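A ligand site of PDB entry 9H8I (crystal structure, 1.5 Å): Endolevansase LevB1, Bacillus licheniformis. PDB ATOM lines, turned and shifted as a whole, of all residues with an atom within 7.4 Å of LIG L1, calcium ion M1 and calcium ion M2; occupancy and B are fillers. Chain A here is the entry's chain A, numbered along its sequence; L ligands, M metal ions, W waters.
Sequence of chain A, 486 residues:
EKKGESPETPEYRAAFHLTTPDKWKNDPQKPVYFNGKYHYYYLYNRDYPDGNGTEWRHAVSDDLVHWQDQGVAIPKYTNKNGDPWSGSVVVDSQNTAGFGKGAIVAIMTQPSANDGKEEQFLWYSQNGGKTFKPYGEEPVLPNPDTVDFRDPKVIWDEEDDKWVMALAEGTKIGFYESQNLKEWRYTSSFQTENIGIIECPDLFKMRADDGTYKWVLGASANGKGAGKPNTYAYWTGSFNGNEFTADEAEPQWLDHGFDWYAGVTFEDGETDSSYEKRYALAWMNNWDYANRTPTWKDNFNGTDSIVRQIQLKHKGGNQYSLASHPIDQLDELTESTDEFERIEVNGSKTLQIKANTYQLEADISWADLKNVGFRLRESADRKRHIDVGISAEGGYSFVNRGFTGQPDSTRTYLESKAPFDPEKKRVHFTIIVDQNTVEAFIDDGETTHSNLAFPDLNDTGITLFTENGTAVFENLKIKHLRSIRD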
ATOM      1  N   ALA A 221      -1.994   4.272   3.780  1.00  0.00           N
ATOM      2  CA  ALA A 221      -2.196   4.510   2.355  1.00  0.00           C
ATOM      3  C   ALA A 221      -1.984   6.011   2.142  1.00  0.00           C
ATOM      4  O   ALA A 221      -1.675   6.735   3.083  1.00  0.00           O
ATOM      5  CB  ALA A 221      -3.580   4.087   1.948  1.00  0.00           C
ATOM      6  N   ASN A 222      -2.066   6.397   0.875  1.00  0.00           N
ATOM      7  CA  ASN A 222      -1.776   7.786   0.511  1.00  0.00           C
ATOM      8  C   ASN A 222      -2.733   8.202  -0.600  1.00  0.00           C
ATOM      9  O   ASN A 222      -2.481   8.039  -1.815  1.00  0.00           O
ATOM     10  CB  ASN A 222      -0.306   7.965   0.116  1.00  0.00           C
ATOM     11  CG  ASN A 222       0.088   9.426   0.088  1.00  0.00           C
ATOM     12  OD1 ASN A 222      -0.798  10.310   0.085  1.00  0.00           O
ATOM     13  ND2 ASN A 222       1.389   9.686   0.136  1.00  0.00           N
ATOM     14  N   LYS A 224      -3.557  11.347  -1.262  1.00  0.00           N
ATOM     15  CA  LYS A 224      -3.419  12.771  -1.495  1.00  0.00           C
ATOM     16  C   LYS A 224      -3.759  13.155  -2.931  1.00  0.00           C
ATOM     17  O   LYS A 224      -4.202  14.303  -3.109  1.00  0.00           O
ATOM     18  CB  LYS A 224      -2.006  13.245  -1.120  1.00  0.00           C
ATOM     19  CG  LYS A 224      -0.822  12.838  -2.026  1.00  0.00           C
ATOM     20  CD  LYS A 224       0.487  13.450  -1.509  1.00  0.00           C
ATOM     21  CE  LYS A 224       1.629  13.238  -2.441  1.00  0.00           C
ATOM     22  NZ  LYS A 224       2.908  13.769  -1.905  1.00  0.00           N
ATOM     23  N   PRO A 229      -6.979  11.491   2.754  1.00  0.00           N
ATOM     24  CA  PRO A 229      -5.850  11.431   3.676  1.00  0.00           C
ATOM     25  C   PRO A 229      -4.718  10.492   3.293  1.00  0.00           C
ATOM     26  O   PRO A 229      -4.864   9.626   2.414  1.00  0.00           O
ATOM     27  CB  PRO A 229      -6.493  10.964   4.978  1.00  0.00           C
ATOM     28  CG  PRO A 229      -7.974  11.384   4.865  1.00  0.00           C
ATOM     29  CD  PRO A 229      -8.240  11.121   3.391  1.00  0.00           C
ATOM     30  N   ASN A 230      -3.628  10.646   4.062  1.00  0.00           N
ATOM     31  CA  ASN A 230      -2.435   9.825   3.988  1.00  0.00           C
ATOM     32  C   ASN A 230      -2.266   9.129   5.339  1.00  0.00           C
ATOM     33  O   ASN A 230      -1.210   9.248   5.943  1.00  0.00           O
ATOM     34  CB  ASN A 230      -1.277  10.754   3.629  1.00  0.00           C
ATOM     35  CG  ASN A 230       0.120  10.177   3.634  1.00  0.00           C
ATOM     36  OD1 ASN A 230       1.079  10.941   3.877  1.00  0.00           O
ATOM     37  ND2 ASN A 230       0.304   8.907   3.325  1.00  0.00           N
ATOM     38  N   THR A 231      -3.314   8.509   5.859  1.00  0.00           N
ATOM     39  CA  THR A 231      -3.311   7.956   7.208  1.00  0.00           C
ATOM     40  C   THR A 231      -3.608   6.458   7.166  1.00  0.00           C
ATOM     41  O   THR A 231      -2.834   5.696   6.636  1.00  0.00           O
ATOM     42  CB  THR A 231      -4.276   8.747   8.094  1.00  0.00           C
ATOM     43  OG1 THR A 231      -5.582   8.632   7.525  1.00  0.00           O
ATOM     44  CG2 THR A 231      -3.838  10.193   8.178  1.00  0.00           C
ATOM     45  N   GLY A 257      -6.365  14.046   9.753  1.00  0.00           N
ATOM     46  CA  GLY A 257      -5.176  14.896   9.911  1.00  0.00           C
ATOM     47  C   GLY A 257      -4.097  14.529   8.908  1.00  0.00           C
ATOM     48  O   GLY A 257      -4.147  13.538   8.147  1.00  0.00           O
ATOM     49  N   PHE A 258      -3.041  15.367   8.929  1.00  0.00           N
ATOM     50  CA  PHE A 258      -1.869  15.117   8.093  1.00  0.00           C
ATOM     51  C   PHE A 258      -0.931  14.020   8.621  1.00  0.00           C
ATOM     52  O   PHE A 258      -0.259  13.386   7.805  1.00  0.00           O
ATOM     53  CB  PHE A 258      -1.069  16.392   7.911  1.00  0.00           C
ATOM     54  CG  PHE A 258      -1.825  17.454   7.142  1.00  0.00           C
ATOM     55  CD1 PHE A 258      -2.444  17.156   5.948  1.00  0.00           C
ATOM     56  CD2 PHE A 258      -1.967  18.711   7.697  1.00  0.00           C
ATOM     57  CE1 PHE A 258      -3.147  18.140   5.270  1.00  0.00           C
ATOM     58  CE2 PHE A 258      -2.645  19.717   7.002  1.00  0.00           C
ATOM     59  CZ  PHE A 258      -3.240  19.428   5.824  1.00  0.00           C
ATOM     60  N   ASP A 259      -0.960  13.755   9.929  1.00  0.00           N
ATOM     61  CA  ASP A 259       0.092  13.046  10.650  1.00  0.00           C
ATOM     62  C   ASP A 259      -0.472  11.902  11.495  1.00  0.00           C
ATOM     63  O   ASP A 259      -0.675  12.040  12.726  1.00  0.00           O
ATOM     64  CB  ASP A 259       0.930  14.054  11.433  1.00  0.00           C
ATOM     65  CG  ASP A 259       1.446  15.187  10.566  1.00  0.00           C
ATOM     66  OD1 ASP A 259       2.050  14.897   9.491  1.00  0.00           O
ATOM     67  OD2 ASP A 259       1.183  16.360  10.939  1.00  0.00           O
ATOM     68  N   TRP A 260      -0.712  10.750  10.832  1.00  0.00           N
ATOM     69  CA  TRP A 260      -1.162   9.547  11.551  1.00  0.00           C
ATOM     70  C   TRP A 260      -0.860   8.345  10.660  1.00  0.00           C
ATOM     71  O   TRP A 260      -1.774   7.803  10.012  1.00  0.00           O
ATOM     72  CB  TRP A 260      -2.646   9.666  11.967  1.00  0.00           C
ATOM     73  CG  TRP A 260      -3.022   8.898  13.183  1.00  0.00           C
ATOM     74  CD1 TRP A 260      -2.800   9.310  14.472  1.00  0.00           C
ATOM     75  CD2 TRP A 260      -3.628   7.578  13.267  1.00  0.00           C
ATOM     76  NE1 TRP A 260      -3.164   8.323  15.355  1.00  0.00           N
ATOM     77  CE2 TRP A 260      -3.732   7.287  14.635  1.00  0.00           C
ATOM     78  CE3 TRP A 260      -4.065   6.653  12.305  1.00  0.00           C
ATOM     79  CZ2 TRP A 260      -4.252   6.067  15.073  1.00  0.00           C
ATOM     80  CZ3 TRP A 260      -4.555   5.442  12.741  1.00  0.00           C
ATOM     81  CH2 TRP A 260      -4.648   5.159  14.113  1.00  0.00           C
ATOM     82  N   TYR A 261       0.435   7.978  10.575  1.00  0.00           N
ATOM     83  CA  TYR A 261       0.893   7.005   9.593  1.00  0.00           C
ATOM     84  C   TYR A 261       1.387   5.709  10.271  1.00  0.00           C
ATOM     85  O   TYR A 261       1.820   5.737  11.441  1.00  0.00           O
ATOM     86  CB  TYR A 261       1.967   7.576   8.684  1.00  0.00           C
ATOM     87  CG  TYR A 261       2.107   6.710   7.458  1.00  0.00           C
ATOM     88  CD1 TYR A 261       1.182   6.761   6.411  1.00  0.00           C
ATOM     89  CD2 TYR A 261       3.185   5.814   7.295  1.00  0.00           C
ATOM     90  CE1 TYR A 261       1.306   5.966   5.290  1.00  0.00           C
ATOM     91  CE2 TYR A 261       3.293   4.997   6.187  1.00  0.00           C
ATOM     92  CZ  TYR A 261       2.340   5.041   5.185  1.00  0.00           C
ATOM     93  OH  TYR A 261       2.408   4.271   4.093  1.00  0.00           O
ATOM     94  N   ASN A 285       5.116  11.955  11.552  1.00  0.00           N
ATOM     95  CA  ASN A 285       6.423  11.954  10.954  1.00  0.00           C
ATOM     96  C   ASN A 285       6.830  13.388  10.606  1.00  0.00           C
ATOM     97  O   ASN A 285       6.292  13.974   9.683  1.00  0.00           O
ATOM     98  CB  ASN A 285       6.441  11.064   9.734  1.00  0.00           C
ATOM     99  CG  ASN A 285       7.819  10.807   9.208  1.00  0.00           C
ATOM    100  OD1 ASN A 285       8.739  11.636   9.298  1.00  0.00           O
ATOM    101  ND2 ASN A 285       8.007   9.612   8.681  1.00  0.00           N
ATOM    102  N   ASN A 286       7.812  13.936  11.309  1.00  0.00           N
ATOM    103  CA  ASN A 286       8.365  15.255  11.042  1.00  0.00           C
ATOM    104  C   ASN A 286       9.434  15.226   9.939  1.00  0.00           C
ATOM    105  O   ASN A 286       9.406  16.027   9.029  1.00  0.00           O
ATOM    106  CB  ASN A 286       9.006  15.818  12.298  1.00  0.00           C
ATOM    107  CG  ASN A 286       9.456  17.259  12.100  1.00  0.00           C
ATOM    108  OD1 ASN A 286       8.722  18.130  11.612  1.00  0.00           O
ATOM    109  ND2 ASN A 286      10.748  17.508  12.328  1.00  0.00           N
ATOM    110  N   TRP A 287      10.325  14.235   9.937  1.00  0.00           N
ATOM    111  CA  TRP A 287      11.417  14.203   8.983  1.00  0.00           C
ATOM    112  C   TRP A 287      10.914  14.072   7.550  1.00  0.00           C
ATOM    113  O   TRP A 287      11.559  14.568   6.621  1.00  0.00           O
ATOM    114  CB  TRP A 287      12.416  13.092   9.287  1.00  0.00           C
ATOM    115  CG  TRP A 287      13.425  13.438  10.358  1.00  0.00           C
ATOM    116  CD1 TRP A 287      13.614  14.621  10.997  1.00  0.00           C
ATOM    117  CD2 TRP A 287      14.388  12.520  10.908  1.00  0.00           C
ATOM    118  NE1 TRP A 287      14.653  14.498  11.918  1.00  0.00           N
ATOM    119  CE2 TRP A 287      15.130  13.227  11.864  1.00  0.00           C
ATOM    120  CE3 TRP A 287      14.669  11.174  10.663  1.00  0.00           C
ATOM    121  CZ2 TRP A 287      16.173  12.631  12.583  1.00  0.00           C
ATOM    122  CZ3 TRP A 287      15.700  10.585  11.377  1.00  0.00           C
ATOM    123  CH2 TRP A 287      16.421  11.297  12.332  1.00  0.00           C
ATOM    124  N   ASP A 288       9.769  13.401   7.334  1.00  0.00           N
ATOM    125  CA  ASP A 288       9.315  13.190   5.979  1.00  0.00           C
ATOM    126  C   ASP A 288       8.858  14.482   5.283  1.00  0.00           C
ATOM    127  O   ASP A 288       8.585  14.471   4.058  1.00  0.00           O
ATOM    128  CB  ASP A 288       8.215  12.123   5.966  1.00  0.00           C
ATOM    129  CG  ASP A 288       7.972  11.586   4.578  1.00  0.00           C
ATOM    130  OD1 ASP A 288       8.951  11.176   3.901  1.00  0.00           O
ATOM    131  OD2 ASP A 288       6.783  11.595   4.118  1.00  0.00           O
ATOM    132  N   TYR A 289       8.658  15.569   6.068  1.00  0.00           N
ATOM    133  CA  TYR A 289       8.353  16.838   5.424  1.00  0.00           C
ATOM    134  C   TYR A 289       9.584  17.569   4.876  1.00  0.00           C
ATOM    135  O   TYR A 289       9.387  18.605   4.226  1.00  0.00           O
ATOM    136  CB  TYR A 289       7.700  17.761   6.442  1.00  0.00           C
ATOM    137  CG  TYR A 289       6.259  17.477   6.767  1.00  0.00           C
ATOM    138  CD1 TYR A 289       5.252  18.017   5.982  1.00  0.00           C
ATOM    139  CD2 TYR A 289       5.927  16.645   7.834  1.00  0.00           C
ATOM    140  CE1 TYR A 289       3.915  17.733   6.269  1.00  0.00           C
ATOM    141  CE2 TYR A 289       4.608  16.362   8.116  1.00  0.00           C
ATOM    142  CZ  TYR A 289       3.605  16.960   7.356  1.00  0.00           C
ATOM    143  OH  TYR A 289       2.279  16.683   7.647  1.00  0.00           O
ATOM    144  N   ALA A 290      10.804  17.127   5.161  1.00  0.00           N
ATOM    145  CA  ALA A 290      12.018  17.831   4.693  1.00  0.00           C
ATOM    146  C   ALA A 290      11.952  17.978   3.173  1.00  0.00           C
ATOM    147  O   ALA A 290      11.631  17.024   2.459  1.00  0.00           O
ATOM    148  CB  ALA A 290      13.215  16.999   5.097  1.00  0.00           C
ATOM    149  N   ARG A 401      -2.867  24.818  10.901  1.00  0.00           N
ATOM    150  CA  ARG A 401      -1.597  25.089  11.561  1.00  0.00           C
ATOM    151  C   ARG A 401      -0.804  26.160  10.808  1.00  0.00           C
ATOM    152  O   ARG A 401       0.375  26.381  11.107  1.00  0.00           O
ATOM    153  CB  ARG A 401      -0.737  23.808  11.707  1.00  0.00           C
ATOM    154  CG  ARG A 401      -0.261  23.164  10.433  1.00  0.00           C
ATOM    155  CD  ARG A 401       0.264  21.784  10.730  1.00  0.00           C
ATOM    156  NE  ARG A 401       0.722  21.181   9.475  1.00  0.00           N
ATOM    157  CZ  ARG A 401       1.069  19.885   9.326  1.00  0.00           C
ATOM    158  NH1 ARG A 401       1.161  19.162  10.406  1.00  0.00           N
ATOM    159  NH2 ARG A 401       1.315  19.409   8.127  1.00  0.00           N
ATOM    160  N   PRO A 407       5.553  21.898  10.031  1.00  0.00           N
ATOM    161  CA  PRO A 407       6.717  21.234   9.429  1.00  0.00           C
ATOM    162  C   PRO A 407       6.968  21.419   7.935  1.00  0.00           C
ATOM    163  O   PRO A 407       8.022  21.004   7.442  1.00  0.00           O
ATOM    164  CB  PRO A 407       6.407  19.741   9.700  1.00  0.00           C
ATOM    165  CG  PRO A 407       4.915  19.707   9.624  1.00  0.00           C
ATOM    166  CD  PRO A 407       4.448  20.958  10.390  1.00  0.00           C
ATOM    167  N   ASP A 408       5.996  21.920   7.185  1.00  0.00           N
ATOM    168  CA  ASP A 408       6.069  21.958   5.726  1.00  0.00           C
ATOM    169  C   ASP A 408       6.605  23.300   5.227  1.00  0.00           C
ATOM    170  O   ASP A 408       5.838  24.248   5.143  1.00  0.00           O
ATOM    171  CB  ASP A 408       4.704  21.675   5.130  1.00  0.00           C
ATOM    172  CG  ASP A 408       4.610  21.643   3.619  1.00  0.00           C
ATOM    173  OD1 ASP A 408       5.728  21.697   2.955  1.00  0.00           O
ATOM    174  OD2 ASP A 408       3.480  21.555   3.087  1.00  0.00           O
ATOM    175  N   TYR A 413       0.645  21.676   3.311  1.00  0.00           N
ATOM    176  CA  TYR A 413      -0.100  20.912   4.302  1.00  0.00           C
ATOM    177  C   TYR A 413      -0.368  21.748   5.545  1.00  0.00           C
ATOM    178  O   TYR A 413       0.289  21.598   6.547  1.00  0.00           O
ATOM    179  CB  TYR A 413       0.572  19.556   4.571  1.00  0.00           C
ATOM    180  CG  TYR A 413       0.649  18.740   3.287  1.00  0.00           C
ATOM    181  CD1 TYR A 413      -0.449  18.039   2.794  1.00  0.00           C
ATOM    182  CD2 TYR A 413       1.803  18.696   2.543  1.00  0.00           C
ATOM    183  CE1 TYR A 413      -0.412  17.370   1.582  1.00  0.00           C
ATOM    184  CE2 TYR A 413       1.871  17.974   1.354  1.00  0.00           C
ATOM    185  CZ  TYR A 413       0.749  17.306   0.859  1.00  0.00           C
ATOM    186  OH  TYR A 413       0.771  16.645  -0.328  1.00  0.00           O
HETATM  187  N1  LIG L   1       2.884  14.110   3.538  1.00  0.00           N
HETATM  188  C1  LIG L   1       2.531  13.764   2.174  1.00  0.00           C
HETATM  189  C2  LIG L   1       3.137  12.450   1.657  1.00  0.00           C
HETATM  190  O1  LIG L   1       3.704  11.739   2.577  1.00  0.00           O
HETATM  191  O2  LIG L   1       3.039  12.197   0.437  1.00  0.00           O
HETATM  192  C3  LIG L   1       4.289  14.590   3.562  1.00  0.00           C
HETATM  193  C4  LIG L   1       4.951  14.376   4.890  1.00  0.00           C
HETATM  194  O3  LIG L   1       4.923  12.971   5.289  1.00  0.00           O
HETATM  195  C5  LIG L   1       1.973  15.111   4.120  1.00  0.00           C
HETATM  196  C6  LIG L   1       0.785  14.462   4.763  1.00  0.00           C
HETATM  197  O4  LIG L   1       1.276  13.476   5.716  1.00  0.00           O
HETATM  198  N1  LG2 L   2       6.258   8.098   3.940  1.00  0.00           N
HETATM  199  C1  LG2 L   2       5.941   8.254   5.358  1.00  0.00           C
HETATM  200  C2  LG2 L   2       4.867   9.275   5.742  1.00  0.00           C
HETATM  201  O1  LG2 L   2       4.429  10.066   4.782  1.00  0.00           O
HETATM  202  O2  LG2 L   2       4.448   9.240   6.911  1.00  0.00           O
HETATM  203  C3  LG2 L   2       7.722   7.919   3.761  1.00  0.00           C
HETATM  204  C4  LG2 L   2       8.177   8.250   2.392  1.00  0.00           C
HETATM  205  O3  LG2 L   2       7.825   9.593   2.069  1.00  0.00           O
HETATM  206  C5  LG2 L   2       5.479   6.985   3.335  1.00  0.00           C
HETATM  207  C6  LG2 L   2       4.008   7.260   3.365  1.00  0.00           C
HETATM  208  O4  LG2 L   2       3.708   8.398   2.564  1.00  0.00           O
HETATM  209 CA    CA M   1       2.875  11.881   4.814  1.00  0.00          CA
HETATM  210 CA    CA M   2       5.486  10.181   2.527  1.00  0.00          CA
HETATM  211  O   HOH W   1       5.354  14.671   0.003  1.00  0.00           O
HETATM  212  O   HOH W   2       2.639  11.104   7.154  1.00  0.00           O
HETATM  213  O   HOH W   3       6.363  11.980   1.012  1.00  0.00           O
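O of Phe 258 lies close to O4 of LIG L1. NZ of Lys 224 lies within salt-bridge range of O2 of LIG L1 (2.8 Å). ND2 of Asn 222 lies within hydrogen-bond range of O2 of LIG L1, at 3.0 Å.
The side-chain amide nitrogen of Asn 230 lies close to the side-chain amide nitrogen of Asn 222 (3.5 Å). The backbone carbonyl oxygen (O) of Ala 221 lies within hydrogen-bond range of the side-chain amide nitrogen (ND2) of Asn 230 (2.9 Å). N of Asp 288 is in hydrogen-bond range of OD1 of Asn 285. N of Lys 224 is in hydrogen-bond range of OD1 of Asn 222, 3.2 Å away. OH of Tyr 289 lies within hydrogen-bond range of OD1 of Asp 259 (2.6 Å). The side-chain hydroxyl (OH) of Tyr 289 sits at hydrogen-bond distance from the guanidinium group (NH2) of Arg 401 (2.9 Å). The guanidinium group of Arg 401 sits at hydrogen-bond distance from the backbone carbonyl oxygen of Tyr 413 (2.9 Å). The backbone NH (N) of Tyr 413 sits at hydrogen-bond distance from the side-chain carboxylate (OD2) of Asp 408, at 2.8 Å.
Tyr 289 touches LIG L1 (CE1 to C4, 3.8 Å). CD2 of Tyr 413 touches C5 of LIG L1, 3.9 Å away. Hydrophobic or aromatic side chains that line LIG L1: Tyr 289 and Tyr 413. Seven residues have an atom within 4 Å of LIG L1: Asn 222, Lys 224, Asn 230, Phe 258, Asp 288, Tyr 289 and Tyr 413. Along chain A the residues within 4 Å of LIG L1 span positions 222 to 413. The nearest printed residue that does not touch LIG L1 is Asp 259 (4.1 Å).
Along chain A the residues within 4 Å of calcium ion M1 span positions 230 to 288.
The nearest printed residue that does not touch calcium ion M2 is Asn 230 (4.7 Å).
Calcium ion M1 is bound by the side-chain amide oxygen (OD1) of Asn 230 (2.2 Å), an oxygen (O3) of LIG L1 (2.4 Å), an oxygen (O1) of LG2 L2 (2.4 Å), an oxygen (O1) of LIG L1 (2.4 Å), an oxygen (O4) of LIG L1 (2.4 Å), water W2 (2.5 Å) and a nitrogen (N1) of LIG L1 (2.6 Å). Calcium ion M1 has seven donor atoms within binding distance.
Calcium ion M2 is bound by an oxygen (O1) of LIG L1 (2.4 Å), an oxygen (O3) of LG2 L2 (2.5 Å), the side-chain carboxylate of Asp 288 (2.5 Å), an oxygen (O1) of LG2 L2 (2.5 Å), water W3 (2.5 Å), an oxygen (O4) of LG2 L2 (2.5 Å) and a nitrogen (N1) of LG2 L2 (2.6 Å).
Water W1 lies within hydrogen-bond range of the side-chain amino group (NZ) of Lys 224 and an oxygen (O2) of LIG L1.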
